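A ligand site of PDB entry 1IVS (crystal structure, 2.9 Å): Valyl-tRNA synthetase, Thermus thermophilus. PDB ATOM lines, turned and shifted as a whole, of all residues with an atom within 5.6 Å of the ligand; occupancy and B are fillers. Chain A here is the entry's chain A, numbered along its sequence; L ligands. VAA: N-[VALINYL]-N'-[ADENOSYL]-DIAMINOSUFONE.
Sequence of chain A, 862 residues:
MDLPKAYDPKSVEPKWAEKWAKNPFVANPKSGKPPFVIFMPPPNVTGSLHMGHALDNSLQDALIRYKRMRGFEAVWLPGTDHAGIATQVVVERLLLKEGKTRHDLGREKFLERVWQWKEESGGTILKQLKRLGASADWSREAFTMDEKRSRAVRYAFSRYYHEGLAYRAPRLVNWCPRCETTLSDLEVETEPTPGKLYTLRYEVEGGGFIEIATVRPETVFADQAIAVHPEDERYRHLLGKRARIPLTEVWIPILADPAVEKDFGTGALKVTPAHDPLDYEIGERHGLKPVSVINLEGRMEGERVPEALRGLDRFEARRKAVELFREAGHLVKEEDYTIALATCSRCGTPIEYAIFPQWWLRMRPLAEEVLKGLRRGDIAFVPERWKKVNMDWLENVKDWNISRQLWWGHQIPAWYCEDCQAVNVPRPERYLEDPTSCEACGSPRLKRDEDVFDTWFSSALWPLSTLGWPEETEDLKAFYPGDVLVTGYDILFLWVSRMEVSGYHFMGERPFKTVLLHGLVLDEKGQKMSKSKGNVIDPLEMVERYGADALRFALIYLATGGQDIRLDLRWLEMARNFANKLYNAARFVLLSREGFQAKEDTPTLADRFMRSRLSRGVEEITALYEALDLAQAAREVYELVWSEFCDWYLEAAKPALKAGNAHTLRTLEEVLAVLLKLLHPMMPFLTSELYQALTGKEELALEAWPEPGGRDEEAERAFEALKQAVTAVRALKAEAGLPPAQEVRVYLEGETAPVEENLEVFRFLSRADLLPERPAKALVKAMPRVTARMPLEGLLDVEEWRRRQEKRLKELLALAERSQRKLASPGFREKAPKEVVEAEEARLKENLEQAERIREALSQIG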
ATOM      1  N   PRO A  41      -9.069  10.826  30.501  1.00  0.00           N
ATOM      2  CA  PRO A  41      -9.507  11.835  29.524  1.00  0.00           C
ATOM      3  C   PRO A  41     -10.264  12.867  30.361  1.00  0.00           C
ATOM      4  O   PRO A  41     -11.312  12.568  30.942  1.00  0.00           O
ATOM      5  CB  PRO A  41     -10.411  11.033  28.601  1.00  0.00           C
ATOM      6  CG  PRO A  41     -10.993   9.993  29.536  1.00  0.00           C
ATOM      7  CD  PRO A  41      -9.780   9.550  30.299  1.00  0.00           C
ATOM      8  N   PRO A  42      -9.737  14.091  30.441  1.00  0.00           N
ATOM      9  CA  PRO A  42     -10.342  15.176  31.210  1.00  0.00           C
ATOM     10  C   PRO A  42     -11.739  15.656  30.820  1.00  0.00           C
ATOM     11  O   PRO A  42     -11.935  16.210  29.746  1.00  0.00           O
ATOM     12  CB  PRO A  42      -9.311  16.300  31.092  1.00  0.00           C
ATOM     13  CG  PRO A  42      -8.693  16.023  29.761  1.00  0.00           C
ATOM     14  CD  PRO A  42      -8.487  14.543  29.798  1.00  0.00           C
ATOM     15  N   PRO A  43     -12.732  15.434  31.693  1.00  0.00           N
ATOM     16  CA  PRO A  43     -14.110  15.852  31.448  1.00  0.00           C
ATOM     17  C   PRO A  43     -14.245  17.372  31.183  1.00  0.00           C
ATOM     18  O   PRO A  43     -13.655  18.176  31.901  1.00  0.00           O
ATOM     19  CB  PRO A  43     -14.813  15.433  32.745  1.00  0.00           C
ATOM     20  CG  PRO A  43     -14.113  14.153  33.063  1.00  0.00           C
ATOM     21  CD  PRO A  43     -12.656  14.486  32.825  1.00  0.00           C
ATOM     22  N   ASN A  44     -15.002  17.758  30.166  1.00  0.00           N
ATOM     23  CA  ASN A  44     -15.181  19.177  29.859  1.00  0.00           C
ATOM     24  C   ASN A  44     -15.884  19.912  30.996  1.00  0.00           C
ATOM     25  O   ASN A  44     -16.876  19.426  31.542  1.00  0.00           O
ATOM     26  CB  ASN A  44     -15.980  19.363  28.564  1.00  0.00           C
ATOM     27  CG  ASN A  44     -15.284  18.771  27.345  1.00  0.00           C
ATOM     28  OD1 ASN A  44     -14.118  19.076  27.065  1.00  0.00           O
ATOM     29  ND2 ASN A  44     -16.002  17.942  26.611  1.00  0.00           N
ATOM     30  N   HIS A  50     -22.069  12.409  33.132  1.00  0.00           N
ATOM     31  CA  HIS A  50     -23.249  11.610  32.865  1.00  0.00           C
ATOM     32  C   HIS A  50     -22.805  10.168  32.801  1.00  0.00           C
ATOM     33  O   HIS A  50     -21.611   9.880  32.783  1.00  0.00           O
ATOM     34  CB  HIS A  50     -23.910  12.053  31.556  1.00  0.00           C
ATOM     35  CG  HIS A  50     -23.012  11.939  30.368  1.00  0.00           C
ATOM     36  ND1 HIS A  50     -22.831  12.981  29.485  1.00  0.00           N
ATOM     37  CD2 HIS A  50     -22.275  10.907  29.906  1.00  0.00           C
ATOM     38  CE1 HIS A  50     -22.018  12.587  28.520  1.00  0.00           C
ATOM     39  NE2 HIS A  50     -21.651  11.333  28.751  1.00  0.00           N
ATOM     40  N   GLY A  52     -22.060   8.264  30.793  1.00  0.00           N
ATOM     41  CA  GLY A  52     -20.991   7.921  29.858  1.00  0.00           C
ATOM     42  C   GLY A  52     -19.641   7.974  30.550  1.00  0.00           C
ATOM     43  O   GLY A  52     -18.873   7.013  30.539  1.00  0.00           O
ATOM     44  N   HIS A  53     -19.359   9.123  31.136  1.00  0.00           N
ATOM     45  CA  HIS A  53     -18.124   9.336  31.859  1.00  0.00           C
ATOM     46  C   HIS A  53     -17.961   8.178  32.832  1.00  0.00           C
ATOM     47  O   HIS A  53     -16.878   7.584  32.938  1.00  0.00           O
ATOM     48  CB  HIS A  53     -18.222  10.654  32.627  1.00  0.00           C
ATOM     49  CG  HIS A  53     -18.463  11.850  31.748  1.00  0.00           C
ATOM     50  ND1 HIS A  53     -19.228  12.929  32.145  1.00  0.00           N
ATOM     51  CD2 HIS A  53     -18.022  12.136  30.502  1.00  0.00           C
ATOM     52  CE1 HIS A  53     -19.239  13.830  31.186  1.00  0.00           C
ATOM     53  NE2 HIS A  53     -18.525  13.383  30.172  1.00  0.00           N
ATOM     54  N   LEU A  55     -18.971   5.119  32.761  1.00  0.00           N
ATOM     55  CA  LEU A  55     -18.501   3.889  32.139  1.00  0.00           C
ATOM     56  C   LEU A  55     -17.019   4.015  31.887  1.00  0.00           C
ATOM     57  O   LEU A  55     -16.230   3.108  32.168  1.00  0.00           O
ATOM     58  CB  LEU A  55     -19.201   3.662  30.805  1.00  0.00           C
ATOM     59  CG  LEU A  55     -18.375   2.812  29.839  1.00  0.00           C
ATOM     60  CD1 LEU A  55     -18.298   1.392  30.343  1.00  0.00           C
ATOM     61  CD2 LEU A  55     -18.984   2.862  28.473  1.00  0.00           C
ATOM     62  N   ASP A  56     -16.649   5.164  31.357  1.00  0.00           N
ATOM     63  CA  ASP A  56     -15.269   5.481  31.013  1.00  0.00           C
ATOM     64  C   ASP A  56     -14.283   5.389  32.190  1.00  0.00           C
ATOM     65  O   ASP A  56     -13.266   4.709  32.096  1.00  0.00           O
ATOM     66  CB  ASP A  56     -15.230   6.878  30.414  1.00  0.00           C
ATOM     67  CG  ASP A  56     -13.863   7.262  29.970  1.00  0.00           C
ATOM     68  OD1 ASP A  56     -13.246   6.455  29.229  1.00  0.00           O
ATOM     69  OD2 ASP A  56     -13.406   8.369  30.358  1.00  0.00           O
ATOM     70  N   ASP A  81     -10.957  19.360  31.515  1.00  0.00           N
ATOM     71  CA  ASP A  81     -10.634  20.148  30.321  1.00  0.00           C
ATOM     72  C   ASP A  81     -11.470  21.432  30.239  1.00  0.00           C
ATOM     73  O   ASP A  81     -12.690  21.404  30.430  1.00  0.00           O
ATOM     74  CB  ASP A  81     -10.859  19.290  29.084  1.00  0.00           C
ATOM     75  CG  ASP A  81     -10.419  19.979  27.805  1.00  0.00           C
ATOM     76  OD1 ASP A  81     -10.143  19.269  26.808  1.00  0.00           O
ATOM     77  OD2 ASP A  81     -10.356  21.223  27.790  1.00  0.00           O
ATOM     78  N   THR A 455      -9.253  24.041  21.783  1.00  0.00           N
ATOM     79  CA  THR A 455      -9.240  23.163  22.953  1.00  0.00           C
ATOM     80  C   THR A 455      -8.596  21.846  22.602  1.00  0.00           C
ATOM     81  O   THR A 455      -7.928  21.231  23.424  1.00  0.00           O
ATOM     82  CB  THR A 455     -10.655  22.854  23.464  1.00  0.00           C
ATOM     83  OG1 THR A 455     -11.319  24.078  23.787  1.00  0.00           O
ATOM     84  CG2 THR A 455     -10.587  21.980  24.712  1.00  0.00           C
ATOM     85  N   TRP A 456      -8.823  21.419  21.375  1.00  0.00           N
ATOM     86  CA  TRP A 456      -8.290  20.158  20.920  1.00  0.00           C
ATOM     87  C   TRP A 456      -6.779  20.202  20.723  1.00  0.00           C
ATOM     88  O   TRP A 456      -6.124  19.153  20.706  1.00  0.00           O
ATOM     89  CB  TRP A 456      -9.003  19.709  19.643  1.00  0.00           C
ATOM     90  CG  TRP A 456     -10.448  19.415  19.898  1.00  0.00           C
ATOM     91  CD1 TRP A 456     -11.524  20.164  19.525  1.00  0.00           C
ATOM     92  CD2 TRP A 456     -10.956  18.345  20.699  1.00  0.00           C
ATOM     93  NE1 TRP A 456     -12.678  19.626  20.041  1.00  0.00           N
ATOM     94  CE2 TRP A 456     -12.351  18.510  20.777  1.00  0.00           C
ATOM     95  CE3 TRP A 456     -10.368  17.262  21.367  1.00  0.00           C
ATOM     96  CZ2 TRP A 456     -13.168  17.643  21.496  1.00  0.00           C
ATOM     97  CZ3 TRP A 456     -11.165  16.401  22.078  1.00  0.00           C
ATOM     98  CH2 TRP A 456     -12.559  16.591  22.140  1.00  0.00           C
ATOM     99  N   SER A 459      -5.435  19.599  24.416  1.00  0.00           N
ATOM    100  CA  SER A 459      -5.817  18.245  24.779  1.00  0.00           C
ATOM    101  C   SER A 459      -4.935  17.192  24.117  1.00  0.00           C
ATOM    102  O   SER A 459      -4.776  16.090  24.639  1.00  0.00           O
ATOM    103  CB  SER A 459      -7.269  18.037  24.399  1.00  0.00           C
ATOM    104  OG  SER A 459      -8.064  19.090  24.917  1.00  0.00           O
ATOM    105  N   VAL A 486      -7.722   4.640  27.778  1.00  0.00           N
ATOM    106  CA  VAL A 486      -9.133   4.325  27.817  1.00  0.00           C
ATOM    107  C   VAL A 486      -9.948   5.529  27.359  1.00  0.00           C
ATOM    108  O   VAL A 486      -9.762   6.640  27.854  1.00  0.00           O
ATOM    109  CB  VAL A 486      -9.545   3.944  29.250  1.00  0.00           C
ATOM    110  CG1 VAL A 486     -11.024   3.601  29.302  1.00  0.00           C
ATOM    111  CG2 VAL A 486      -8.718   2.773  29.712  1.00  0.00           C
ATOM    112  N   THR A 487     -10.823   5.295  26.392  1.00  0.00           N
ATOM    113  CA  THR A 487     -11.679   6.343  25.875  1.00  0.00           C
ATOM    114  C   THR A 487     -12.638   5.748  24.842  1.00  0.00           C
ATOM    115  O   THR A 487     -12.379   4.696  24.246  1.00  0.00           O
ATOM    116  CB  THR A 487     -10.867   7.445  25.190  1.00  0.00           C
ATOM    117  OG1 THR A 487     -11.723   8.547  24.872  1.00  0.00           O
ATOM    118  CG2 THR A 487     -10.230   6.921  23.905  1.00  0.00           C
ATOM    119  N   GLY A 488     -13.754   6.438  24.654  1.00  0.00           N
ATOM    120  CA  GLY A 488     -14.739   5.978  23.707  1.00  0.00           C
ATOM    121  C   GLY A 488     -14.466   6.539  22.334  1.00  0.00           C
ATOM    122  O   GLY A 488     -14.243   7.727  22.170  1.00  0.00           O
ATOM    123  N   TYR A 489     -14.515   5.662  21.328  1.00  0.00           N
ATOM    124  CA  TYR A 489     -14.252   6.029  19.949  1.00  0.00           C
ATOM    125  C   TYR A 489     -14.757   7.392  19.517  1.00  0.00           C
ATOM    126  O   TYR A 489     -14.268   7.931  18.538  1.00  0.00           O
ATOM    127  CB  TYR A 489     -14.815   4.958  19.005  1.00  0.00           C
ATOM    128  CG  TYR A 489     -16.319   4.747  19.083  1.00  0.00           C
ATOM    129  CD1 TYR A 489     -17.203   5.823  18.952  1.00  0.00           C
ATOM    130  CD2 TYR A 489     -16.857   3.469  19.278  1.00  0.00           C
ATOM    131  CE1 TYR A 489     -18.593   5.631  19.017  1.00  0.00           C
ATOM    132  CE2 TYR A 489     -18.242   3.269  19.337  1.00  0.00           C
ATOM    133  CZ  TYR A 489     -19.094   4.355  19.206  1.00  0.00           C
ATOM    134  OH  TYR A 489     -20.458   4.184  19.287  1.00  0.00           O
ATOM    135  N   ASP A 490     -15.713   7.980  20.229  1.00  0.00           N
ATOM    136  CA  ASP A 490     -16.213   9.272  19.785  1.00  0.00           C
ATOM    137  C   ASP A 490     -15.117  10.312  19.589  1.00  0.00           C
ATOM    138  O   ASP A 490     -15.297  11.243  18.810  1.00  0.00           O
ATOM    139  CB  ASP A 490     -17.269   9.807  20.735  1.00  0.00           C
ATOM    140  CG  ASP A 490     -16.724  10.160  22.087  1.00  0.00           C
ATOM    141  OD1 ASP A 490     -16.016   9.302  22.660  1.00  0.00           O
ATOM    142  OD2 ASP A 490     -17.009  11.291  22.570  1.00  0.00           O
ATOM    143  N   ILE A 491     -13.982  10.196  20.288  1.00  0.00           N
ATOM    144  CA  ILE A 491     -12.919  11.179  20.080  1.00  0.00           C
ATOM    145  C   ILE A 491     -11.611  10.545  19.577  1.00  0.00           C
ATOM    146  O   ILE A 491     -10.529  11.075  19.813  1.00  0.00           O
ATOM    147  CB  ILE A 491     -12.614  12.015  21.353  1.00  0.00           C
ATOM    148  CG1 ILE A 491     -12.149  11.114  22.497  1.00  0.00           C
ATOM    149  CG2 ILE A 491     -13.837  12.828  21.730  1.00  0.00           C
ATOM    150  CD1 ILE A 491     -11.892  11.862  23.814  1.00  0.00           C
ATOM    151  N   TRP A 495      -8.804  13.573  19.499  1.00  0.00           N
ATOM    152  CA  TRP A 495      -8.016  13.409  20.702  1.00  0.00           C
ATOM    153  C   TRP A 495      -6.946  12.342  20.518  1.00  0.00           C
ATOM    154  O   TRP A 495      -5.771  12.664  20.399  1.00  0.00           O
ATOM    155  CB  TRP A 495      -8.884  13.051  21.912  1.00  0.00           C
ATOM    156  CG  TRP A 495      -8.211  13.406  23.250  1.00  0.00           C
ATOM    157  CD1 TRP A 495      -7.673  14.606  23.581  1.00  0.00           C
ATOM    158  CD2 TRP A 495      -8.066  12.558  24.412  1.00  0.00           C
ATOM    159  NE1 TRP A 495      -7.200  14.573  24.879  1.00  0.00           N
ATOM    160  CE2 TRP A 495      -7.423  13.326  25.403  1.00  0.00           C
ATOM    161  CE3 TRP A 495      -8.403  11.225  24.702  1.00  0.00           C
ATOM    162  CZ2 TRP A 495      -7.122  12.810  26.667  1.00  0.00           C
ATOM    163  CZ3 TRP A 495      -8.094  10.715  25.964  1.00  0.00           C
ATOM    164  CH2 TRP A 495      -7.461  11.505  26.932  1.00  0.00           C
ATOM    165  N   HIS A 518     -13.818   1.850  24.188  1.00  0.00           N
ATOM    166  CA  HIS A 518     -15.067   1.290  24.674  1.00  0.00           C
ATOM    167  C   HIS A 518     -16.195   2.008  23.961  1.00  0.00           C
ATOM    168  O   HIS A 518     -16.008   3.129  23.510  1.00  0.00           O
ATOM    169  CB  HIS A 518     -15.203   1.518  26.186  1.00  0.00           C
ATOM    170  CG  HIS A 518     -15.425   2.943  26.575  1.00  0.00           C
ATOM    171  ND1 HIS A 518     -14.409   3.771  26.984  1.00  0.00           N
ATOM    172  CD2 HIS A 518     -16.548   3.706  26.570  1.00  0.00           C
ATOM    173  CE1 HIS A 518     -14.893   4.978  27.229  1.00  0.00           C
ATOM    174  NE2 HIS A 518     -16.194   4.959  26.981  1.00  0.00           N
ATOM    175  N   GLY A 519     -17.362   1.368  23.872  1.00  0.00           N
ATOM    176  CA  GLY A 519     -18.501   1.965  23.188  1.00  0.00           C
ATOM    177  C   GLY A 519     -19.102   3.172  23.898  1.00  0.00           C
ATOM    178  O   GLY A 519     -18.462   3.794  24.746  1.00  0.00           O
ATOM    179  N   LEU A 520     -20.322   3.532  23.550  1.00  0.00           N
ATOM    180  CA  LEU A 520     -20.937   4.662  24.211  1.00  0.00           C
ATOM    181  C   LEU A 520     -22.273   4.278  24.846  1.00  0.00           C
ATOM    182  O   LEU A 520     -23.020   3.421  24.346  1.00  0.00           O
ATOM    183  CB  LEU A 520     -21.182   5.816  23.219  1.00  0.00           C
ATOM    184  CG  LEU A 520     -20.137   6.128  22.151  1.00  0.00           C
ATOM    185  CD1 LEU A 520     -20.538   7.368  21.372  1.00  0.00           C
ATOM    186  CD2 LEU A 520     -18.801   6.344  22.805  1.00  0.00           C
ATOM    187  N   VAL A 521     -22.576   4.899  25.978  1.00  0.00           N
ATOM    188  CA  VAL A 521     -23.840   4.604  26.617  1.00  0.00           C
ATOM    189  C   VAL A 521     -24.786   5.550  25.918  1.00  0.00           C
ATOM    190  O   VAL A 521     -24.384   6.647  25.507  1.00  0.00           O
ATOM    191  CB  VAL A 521     -23.805   4.870  28.151  1.00  0.00           C
ATOM    192  CG1 VAL A 521     -22.417   4.601  28.698  1.00  0.00           C
ATOM    193  CG2 VAL A 521     -24.274   6.282  28.458  1.00  0.00           C
ATOM    194  N   LEU A 522     -26.040   5.137  25.763  1.00  0.00           N
ATOM    195  CA  LEU A 522     -27.022   5.941  25.076  1.00  0.00           C
ATOM    196  C   LEU A 522     -28.427   5.688  25.598  1.00  0.00           C
ATOM    197  O   LEU A 522     -28.753   4.550  25.962  1.00  0.00           O
ATOM    198  CB  LEU A 522     -26.929   5.659  23.580  1.00  0.00           C
ATOM    199  CG  LEU A 522     -26.416   4.238  23.317  1.00  0.00           C
ATOM    200  CD1 LEU A 522     -27.563   3.271  23.558  1.00  0.00           C
ATOM    201  CD2 LEU A 522     -25.899   4.105  21.903  1.00  0.00           C
ATOM    202  N   LYS A 528     -26.894   8.132  21.303  1.00  0.00           N
ATOM    203  CA  LYS A 528     -25.844   8.601  22.221  1.00  0.00           C
ATOM    204  C   LYS A 528     -26.232   9.577  23.302  1.00  0.00           C
ATOM    205  O   LYS A 528     -27.006  10.513  23.080  1.00  0.00           O
ATOM    206  CB  LYS A 528     -24.697   9.209  21.409  1.00  0.00           C
ATOM    207  CG  LYS A 528     -23.618   9.878  22.257  1.00  0.00           C
ATOM    208  CD  LYS A 528     -22.507  10.451  21.394  1.00  0.00           C
ATOM    209  CE  LYS A 528     -21.450  11.172  22.222  1.00  0.00           C
ATOM    210  NZ  LYS A 528     -20.397  11.784  21.364  1.00  0.00           N
ATOM    211  N   MET A 529     -25.660   9.365  24.491  1.00  0.00           N
ATOM    212  CA  MET A 529     -25.903  10.205  25.647  1.00  0.00           C
ATOM    213  C   MET A 529     -24.947  11.387  25.593  1.00  0.00           C
ATOM    214  O   MET A 529     -23.735  11.215  25.496  1.00  0.00           O
ATOM    215  CB  MET A 529     -25.686   9.419  26.942  1.00  0.00           C
ATOM    216  CG  MET A 529     -25.915  10.252  28.192  1.00  0.00           C
ATOM    217  SD  MET A 529     -26.292   9.291  29.671  1.00  0.00           S
ATOM    218  CE  MET A 529     -28.051   9.415  29.692  1.00  0.00           C
ATOM    219  N   SER A 530     -25.502  12.584  25.662  1.00  0.00           N
ATOM    220  CA  SER A 530     -24.670  13.774  25.611  1.00  0.00           C
ATOM    221  C   SER A 530     -25.428  15.059  25.927  1.00  0.00           C
ATOM    222  O   SER A 530     -26.601  15.225  25.592  1.00  0.00           O
ATOM    223  CB  SER A 530     -24.016  13.866  24.232  1.00  0.00           C
ATOM    224  OG  SER A 530     -24.998  13.778  23.219  1.00  0.00           O
HETATM  225  N   VAA L   1     -12.027  17.311  27.089  1.00  0.00           N
HETATM  226  CA  VAA L   1     -12.260  16.351  25.964  1.00  0.00           C
HETATM  227  CB  VAA L   1     -11.031  15.360  25.772  1.00  0.00           C
HETATM  228  CG1 VAA L   1     -10.810  14.352  26.966  1.00  0.00           C
HETATM  229  CG2 VAA L   1      -9.801  16.138  25.598  1.00  0.00           C
HETATM  230  C   VAA L   1     -13.495  15.475  26.158  1.00  0.00           C
HETATM  231  O   VAA L   1     -13.632  14.461  25.429  1.00  0.00           O
HETATM  232  S   VAA L   1     -15.806  14.915  27.455  1.00  0.00           S
HETATM  233  O1S VAA L   1     -16.646  15.524  28.574  1.00  0.00           O
HETATM  234  O2S VAA L   1     -16.606  14.697  26.238  1.00  0.00           O
HETATM  235  N3S VAA L   1     -14.379  15.867  27.157  1.00  0.00           N
HETATM  236  N5' VAA L   1     -15.453  13.368  28.054  1.00  0.00           N
HETATM  237  C5' VAA L   1     -15.169  12.591  27.022  1.00  0.00           C
HETATM  238  C4' VAA L   1     -14.692  11.377  27.534  1.00  0.00           C
HETATM  239  O4' VAA L   1     -15.809  10.705  28.062  1.00  0.00           O
HETATM  240  C1' VAA L   1     -16.214   9.651  27.117  1.00  0.00           C
HETATM  241  N9  VAA L   1     -17.618   9.746  26.790  1.00  0.00           N
HETATM  242  C4  VAA L   1     -18.463   8.584  26.649  1.00  0.00           C
HETATM  243  N3  VAA L   1     -18.100   7.246  26.790  1.00  0.00           N
HETATM  244  C2  VAA L   1     -19.140   6.394  26.591  1.00  0.00           C
HETATM  245  N1  VAA L   1     -20.413   6.732  26.284  1.00  0.00           N
HETATM  246  C6  VAA L   1     -20.754   8.094  26.151  1.00  0.00           C
HETATM  247  N6  VAA L   1     -22.032   8.405  25.838  1.00  0.00           N
HETATM  248  C5  VAA L   1     -19.740   9.100  26.338  1.00  0.00           C
HETATM  249  N7  VAA L   1     -19.702  10.504  26.278  1.00  0.00           N
HETATM  250  C8  VAA L   1     -18.488  10.806  26.546  1.00  0.00           C
HETATM  251  C2' VAA L   1     -15.244   9.767  25.926  1.00  0.00           C
HETATM  252  O2' VAA L   1     -14.944   8.432  25.458  1.00  0.00           O
HETATM  253  C3' VAA L   1     -14.102  10.489  26.496  1.00  0.00           C
HETATM  254  O3' VAA L   1     -13.182   9.620  27.195  1.00  0.00           O
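The backbone NH (N) of Gly 488 lies within hydrogen-bond range of an oxygen (O2') of the ligand, at 2.5 Å.
An oxygen (O2') of the ligand sits close to the backbone carbonyl oxygen of Gly 488, at 3.4 Å.
An oxygen (O1S) of the ligand lies within hydrogen-bond range of the backbone NH (N) of Asn 44 (3.2 Å).
The side-chain amide nitrogen (ND2) of Asn 44 sits at hydrogen-bond distance from a nitrogen (N3S) of the ligand, 2.7 Å away.
The side-chain carboxylate (OD1) of Asp 81 lies within salt-bridge range of a nitrogen (N) of the ligand (2.7 Å).
The backbone NH (N) of Val 521 lies within hydrogen-bond range of a nitrogen (N1) of the ligand (2.9 Å).
The backbone carbonyl oxygen of Val 521 sits at hydrogen-bond distance from a nitrogen (N6) of the ligand, at 3.0 Å.
A nitrogen (N) of the ligand lies within hydrogen-bond range of the backbone carbonyl oxygen (O) of Pro 42, at 2.9 Å.
OG1 of Thr 487 sits at hydrogen-bond distance from O3' of the ligand, at 2.9 Å.
NE2 of His 518 is in hydrogen-bond range of N3 of the ligand, at 3.0 Å.
OD1 of Asp 490 is in hydrogen-bond range of O2' of the ligand.
A nitrogen (N7) of the ligand is in hydrogen-bond range of a ring nitrogen (NE2) of His 50 (3.3 Å).
NE2 of His 53 lies within hydrogen-bond range of O1S of the ligand.
N6 of the ligand is in hydrogen-bond range of O of Met 529 (3.3 Å).
An oxygen (O3') of the ligand lies within hydrogen-bond range of the side-chain carboxylate of Asp 56 (3.4 Å).
The backbone carbonyl oxygen of Gly 488 lies close to the side-chain carboxylate of Asp 490, at 2.4 Å.
OD1 of Asp 81 is in hydrogen-bond range of OG of Ser 459 (2.8 Å).
The backbone NH (N) of Asp 81 sits at hydrogen-bond distance from the backbone carbonyl oxygen (O) of Pro 43 (3.0 Å).
The backbone carbonyl oxygen of Val 521 sits at hydrogen-bond distance from the backbone NH of Met 529, 3.2 Å away.
The backbone carbonyl oxygen of Thr 487 lies within hydrogen-bond range of the backbone NH of His 518 (3.2 Å).
OD2 of Asp 490 lies within salt-bridge range of NZ of Lys 528, 3.6 Å away.
The indole nitrogen of Trp 495 lies within hydrogen-bond range of the backbone carbonyl oxygen of Ser 459 (2.9 Å).
OG of Ser 459 sits at hydrogen-bond distance from O of Thr 455.
Residues that only touch the ligand: Leu 520 (3.0 Å), Trp 495 (3.1 Å), Pro 41 (3.2 Å), Gly 519 (3.3 Å), Ser 459 (3.4 Å), Ile 491 (3.5 Å), Gly 52 (3.7 Å), Trp 456 (3.8 Å) and Pro 43 (3.8 Å).
Hydrophobic or aromatic side chains within 4 Å of the ligand: Pro 41, Pro 42, His 50, His 53, Trp 456, Ile 491, Trp 495, His 518, Leu 520, Val 521 and Met 529.
Within 4 Å of the ligand: Pro 41, Pro 42, Pro 43, Asn 44, His 50, Gly 52, His 53, Asp 56, Asp 81, Trp 456, Ser 459, Thr 487, Gly 488, Asp 490, Ile 491, Trp 495, His 518, Gly 519, Leu 520, Val 521 and Met 529.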
